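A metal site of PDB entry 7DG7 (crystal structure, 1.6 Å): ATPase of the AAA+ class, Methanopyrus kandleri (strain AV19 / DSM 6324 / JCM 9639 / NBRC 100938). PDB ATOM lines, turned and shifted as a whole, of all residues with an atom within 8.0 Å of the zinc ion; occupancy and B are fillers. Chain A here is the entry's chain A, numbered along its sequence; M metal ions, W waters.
The side-chain carboxylate (OD1) of Asp 71 sits close to the backbone NH (N) of Gly 21, 3.3 Å away. The backbone NH (N) of Tyr 73 sits at hydrogen-bond distance from the side-chain carboxylate (OD2) of Asp 71 (3.0 Å). The side-chain amino group (NZ) of Lys 22 lies within salt-bridge range of the side-chain carboxylate (OD1) of Asp 19 (2.9 Å).
Merely in contact with the zinc ion: Arg 23 (3.8 Å).
OE2 of Glu 74 binds the zinc ion (1.9 Å). The zinc ion is bound by OD1 of Asp 71. The backbone carbonyl oxygen (O) of Lys 22 is bound to the zinc ion (2.1 Å). The zinc ion is bound by water W1 (2.2 Å). Slightly farther from the zinc ion lies OD2 of Asp 71 (2.8 Å).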
ATOM      1  N   ALA A  15     -26.490 -15.244  19.846  1.00  0.00           N
ATOM      2  CA  ALA A  15     -27.696 -14.475  19.572  1.00  0.00           C
ATOM      3  C   ALA A  15     -28.762 -15.335  18.903  1.00  0.00           C
ATOM      4  O   ALA A  15     -28.456 -16.270  18.156  1.00  0.00           O
ATOM      5  CB  ALA A  15     -27.385 -13.282  18.662  1.00  0.00           C
ATOM      6  N   ASP A  19     -31.657 -11.361  15.929  1.00  0.00           N
ATOM      7  CA  ASP A  19     -30.815 -10.274  16.428  1.00  0.00           C
ATOM      8  C   ASP A  19     -29.437 -10.224  15.773  1.00  0.00           C
ATOM      9  O   ASP A  19     -28.675  -9.294  16.043  1.00  0.00           O
ATOM     10  CB  ASP A  19     -30.687 -10.408  17.956  1.00  0.00           C
ATOM     11  CG  ASP A  19     -32.062 -10.395  18.655  1.00  0.00           C
ATOM     12  OD1 ASP A  19     -32.885  -9.499  18.304  1.00  0.00           O
ATOM     13  OD2 ASP A  19     -32.347 -11.287  19.493  1.00  0.00           O
ATOM     14  N   VAL A  20     -29.106 -11.203  14.920  1.00  0.00           N
ATOM     15  CA  VAL A  20     -27.838 -11.211  14.221  1.00  0.00           C
ATOM     16  C   VAL A  20     -27.763 -10.011  13.289  1.00  0.00           C
ATOM     17  O   VAL A  20     -28.718  -9.707  12.556  1.00  0.00           O
ATOM     18  CB  VAL A  20     -27.664 -12.532  13.485  1.00  0.00           C
ATOM     19  CG1 VAL A  20     -26.434 -12.498  12.592  1.00  0.00           C
ATOM     20  CG2 VAL A  20     -27.628 -13.692  14.493  1.00  0.00           C
ATOM     21  N   GLY A  21     -26.614  -9.336  13.305  1.00  0.00           N
ATOM     22  CA  GLY A  21     -26.402  -8.122  12.547  1.00  0.00           C
ATOM     23  C   GLY A  21     -26.922  -6.862  13.196  1.00  0.00           C
ATOM     24  O   GLY A  21     -26.982  -5.823  12.531  1.00  0.00           O
ATOM     25  N   LYS A  22     -27.337  -6.932  14.462  1.00  0.00           N
ATOM     26  CA  LYS A  22     -27.668  -5.765  15.267  1.00  0.00           C
ATOM     27  C   LYS A  22     -26.501  -5.477  16.201  1.00  0.00           C
ATOM     28  O   LYS A  22     -25.914  -6.396  16.796  1.00  0.00           O
ATOM     29  CB  LYS A  22     -28.900  -6.008  16.124  1.00  0.00           C
ATOM     30  CG  LYS A  22     -30.179  -6.287  15.391  1.00  0.00           C
ATOM     31  CD  LYS A  22     -31.317  -6.518  16.387  1.00  0.00           C
ATOM     32  CE  LYS A  22     -32.650  -6.750  15.671  1.00  0.00           C
ATOM     33  NZ  LYS A  22     -33.678  -7.377  16.573  1.00  0.00           N
ATOM     34  N   ARG A  23     -26.230  -4.187  16.347  1.00  0.00           N
ATOM     35  CA  ARG A  23     -25.183  -3.868  17.338  1.00  0.00           C
ATOM     36  C   ARG A  23     -25.812  -3.920  18.729  1.00  0.00           C
ATOM     37  O   ARG A  23     -25.943  -2.912  19.435  1.00  0.00           O
ATOM     38  CB  ARG A  23     -24.562  -2.502  17.055  1.00  0.00           C
ATOM     39  CG  ARG A  23     -23.798  -2.418  15.745  1.00  0.00           C
ATOM     40  CD  ARG A  23     -23.262  -1.036  15.433  1.00  0.00           C
ATOM     41  NE  ARG A  23     -22.270  -0.593  16.410  1.00  0.00           N
ATOM     42  CZ  ARG A  23     -21.734   0.620  16.424  1.00  0.00           C
ATOM     43  NH1 ARG A  23     -22.086   1.521  15.521  1.00  0.00           N
ATOM     44  NH2 ARG A  23     -20.825   0.932  17.352  1.00  0.00           N
ATOM     45  N   ALA A  24     -26.232  -4.981  19.218  1.00  0.00           N
ATOM     46  CA  ALA A  24     -27.088  -5.047  20.389  1.00  0.00           C
ATOM     47  C   ALA A  24     -26.929  -6.403  21.043  1.00  0.00           C
ATOM     48  O   ALA A  24     -26.659  -7.402  20.371  1.00  0.00           O
ATOM     49  CB  ALA A  24     -28.563  -4.835  20.001  1.00  0.00           C
ATOM     50  N   VAL A  25     -27.142  -6.444  22.367  1.00  0.00           N
ATOM     51  CA  VAL A  25     -27.084  -7.691  23.131  1.00  0.00           C
ATOM     52  C   VAL A  25     -28.305  -7.795  24.022  1.00  0.00           C
ATOM     53  O   VAL A  25     -28.875  -6.782  24.440  1.00  0.00           O
ATOM     54  CB  VAL A  25     -25.796  -7.759  23.982  1.00  0.00           C
ATOM     55  CG1 VAL A  25     -24.552  -7.662  23.095  1.00  0.00           C
ATOM     56  CG2 VAL A  25     -25.815  -6.624  24.991  1.00  0.00           C
ATOM     57  N   VAL A  52     -18.777  -2.004  22.239  1.00  0.00           N
ATOM     58  CA  VAL A  52     -19.970  -1.400  22.798  1.00  0.00           C
ATOM     59  C   VAL A  52     -21.165  -1.922  22.018  1.00  0.00           C
ATOM     60  O   VAL A  52     -21.055  -2.317  20.856  1.00  0.00           O
ATOM     61  CB  VAL A  52     -19.952   0.149  22.744  1.00  0.00           C
ATOM     62  CG1 VAL A  52     -18.794   0.694  23.557  1.00  0.00           C
ATOM     63  CG2 VAL A  52     -19.880   0.615  21.307  1.00  0.00           C
ATOM     64  N   ALA A  53     -22.313  -1.955  22.699  1.00  0.00           N
ATOM     65  CA  ALA A  53     -23.556  -2.386  22.043  1.00  0.00           C
ATOM     66  C   ALA A  53     -24.749  -1.861  22.827  1.00  0.00           C
ATOM     67  O   ALA A  53     -24.659  -1.488  23.993  1.00  0.00           O
ATOM     68  CB  ALA A  53     -23.620  -3.909  21.916  1.00  0.00           C
ATOM     69  N   ARG A  69     -26.604 -12.468  25.424  1.00  0.00           N
ATOM     70  CA  ARG A  69     -26.645 -13.040  24.090  1.00  0.00           C
ATOM     71  C   ARG A  69     -26.018 -12.072  23.100  1.00  0.00           C
ATOM     72  O   ARG A  69     -26.433 -10.908  23.006  1.00  0.00           O
ATOM     73  CB  ARG A  69     -28.080 -13.402  23.685  1.00  0.00           C
ATOM     74  CG  ARG A  69     -28.609 -14.648  24.418  1.00  0.00           C
ATOM     75  CD  ARG A  69     -29.766 -15.302  23.695  1.00  0.00           C
ATOM     76  NE  ARG A  69     -30.297 -16.442  24.457  1.00  0.00           N
ATOM     77  CZ  ARG A  69     -29.802 -17.667  24.398  1.00  0.00           C
ATOM     78  NH1 ARG A  69     -28.762 -17.947  23.610  1.00  0.00           N
ATOM     79  NH2 ARG A  69     -30.369 -18.635  25.123  1.00  0.00           N
ATOM     80  N   MET A  70     -25.032 -12.563  22.355  1.00  0.00           N
ATOM     81  CA  MET A  70     -24.216 -11.766  21.448  1.00  0.00           C
ATOM     82  C   MET A  70     -24.022 -12.485  20.124  1.00  0.00           C
ATOM     83  O   MET A  70     -23.697 -13.669  20.102  1.00  0.00           O
ATOM     84  CB  MET A  70     -22.824 -11.516  22.073  1.00  0.00           C
ATOM     85  CG  MET A  70     -22.941 -10.872  23.404  1.00  0.00           C
ATOM     86  SD  MET A  70     -21.409 -10.435  24.231  1.00  0.00           S
ATOM     87  CE  MET A  70     -20.156 -10.566  22.991  1.00  0.00           C
ATOM     88  N   ASP A  71     -24.168 -11.757  19.005  1.00  0.00           N
ATOM     89  CA  ASP A  71     -23.858 -12.352  17.724  1.00  0.00           C
ATOM     90  C   ASP A  71     -22.345 -12.388  17.487  1.00  0.00           C
ATOM     91  O   ASP A  71     -21.550 -11.970  18.328  1.00  0.00           O
ATOM     92  CB  ASP A  71     -24.577 -11.600  16.587  1.00  0.00           C
ATOM     93  CG  ASP A  71     -24.134 -10.142  16.465  1.00  0.00           C
ATOM     94  OD1 ASP A  71     -25.013  -9.289  16.158  1.00  0.00           O
ATOM     95  OD2 ASP A  71     -22.922  -9.859  16.656  1.00  0.00           O
ATOM     96  N   LYS A  72     -21.973 -12.883  16.303  1.00  0.00           N
ATOM     97  CA  LYS A  72     -20.569 -13.173  16.020  1.00  0.00           C
ATOM     98  C   LYS A  72     -19.738 -11.899  16.007  1.00  0.00           C
ATOM     99  O   LYS A  72     -18.578 -11.895  16.426  1.00  0.00           O
ATOM    100  CB  LYS A  72     -20.453 -13.918  14.697  1.00  0.00           C
ATOM    101  CG  LYS A  72     -19.139 -14.632  14.468  1.00  0.00           C
ATOM    102  CD  LYS A  72     -19.066 -15.261  13.070  1.00  0.00           C
ATOM    103  CE  LYS A  72     -19.914 -16.541  12.963  1.00  0.00           C
ATOM    104  NZ  LYS A  72     -20.221 -16.937  11.518  1.00  0.00           N
ATOM    105  N   TYR A  73     -20.304 -10.802  15.487  1.00  0.00           N
ATOM    106  CA  TYR A  73     -19.529  -9.573  15.414  1.00  0.00           C
ATOM    107  C   TYR A  73     -19.200  -9.056  16.813  1.00  0.00           C
ATOM    108  O   TYR A  73     -18.046  -8.711  17.107  1.00  0.00           O
ATOM    109  CB  TYR A  73     -20.292  -8.538  14.574  1.00  0.00           C
ATOM    110  CG  TYR A  73     -19.496  -7.278  14.349  1.00  0.00           C
ATOM    111  CD1 TYR A  73     -18.201  -7.328  13.853  1.00  0.00           C
ATOM    112  CD2 TYR A  73     -20.047  -6.038  14.647  1.00  0.00           C
ATOM    113  CE1 TYR A  73     -17.483  -6.165  13.637  1.00  0.00           C
ATOM    114  CE2 TYR A  73     -19.326  -4.872  14.444  1.00  0.00           C
ATOM    115  CZ  TYR A  73     -18.051  -4.951  13.937  1.00  0.00           C
ATOM    116  OH  TYR A  73     -17.341  -3.785  13.744  1.00  0.00           O
ATOM    117  N   GLU A  74     -20.192  -9.006  17.700  1.00  0.00           N
ATOM    118  CA  GLU A  74     -19.937  -8.571  19.081  1.00  0.00           C
ATOM    119  C   GLU A  74     -18.983  -9.509  19.805  1.00  0.00           C
ATOM    120  O   GLU A  74     -18.123  -9.066  20.582  1.00  0.00           O
ATOM    121  CB  GLU A  74     -21.262  -8.471  19.855  1.00  0.00           C
ATOM    122  CG  GLU A  74     -21.879  -7.058  19.818  1.00  0.00           C
ATOM    123  CD  GLU A  74     -22.437  -6.693  18.456  1.00  0.00           C
ATOM    124  OE1 GLU A  74     -21.972  -5.706  17.839  1.00  0.00           O
ATOM    125  OE2 GLU A  74     -23.329  -7.403  17.982  1.00  0.00           O
ATOM    126  N   ARG A  75     -19.128 -10.825  19.585  1.00  0.00           N
ATOM    127  CA  ARG A  75     -18.203 -11.751  20.238  1.00  0.00           C
ATOM    128  C   ARG A  75     -16.778 -11.526  19.749  1.00  0.00           C
ATOM    129  O   ARG A  75     -15.840 -11.512  20.550  1.00  0.00           O
ATOM    130  CB  ARG A  75     -18.637 -13.200  20.001  1.00  0.00           C
ATOM    131  CG  ARG A  75     -19.920 -13.552  20.730  1.00  0.00           C
ATOM    132  CD  ARG A  75     -20.219 -15.029  20.705  1.00  0.00           C
ATOM    133  NE  ARG A  75     -20.037 -15.728  19.431  1.00  0.00           N
ATOM    134  CZ  ARG A  75     -21.012 -15.967  18.547  1.00  0.00           C
ATOM    135  NH1 ARG A  75     -22.238 -15.524  18.771  1.00  0.00           N
ATOM    136  NH2 ARG A  75     -20.750 -16.648  17.429  1.00  0.00           N
ATOM    137  N   ASN A  77     -15.558  -8.678  18.614  1.00  0.00           N
ATOM    138  CA  ASN A  77     -15.033  -7.406  19.100  1.00  0.00           C
ATOM    139  C   ASN A  77     -14.820  -7.387  20.597  1.00  0.00           C
ATOM    140  O   ASN A  77     -14.037  -6.576  21.081  1.00  0.00           O
ATOM    141  CB  ASN A  77     -15.948  -6.254  18.706  1.00  0.00           C
ATOM    142  CG  ASN A  77     -16.076  -6.091  17.209  1.00  0.00           C
ATOM    143  OD1 ASN A  77     -15.216  -6.535  16.446  1.00  0.00           O
ATOM    144  ND2 ASN A  77     -17.164  -5.452  16.781  1.00  0.00           N
HETATM  145 ZN    ZN M   1     -24.221  -7.462  16.284  1.00  0.00          ZN
HETATM  146  O   HOH W   1     -23.689  -6.458  14.455  1.00  0.00           O
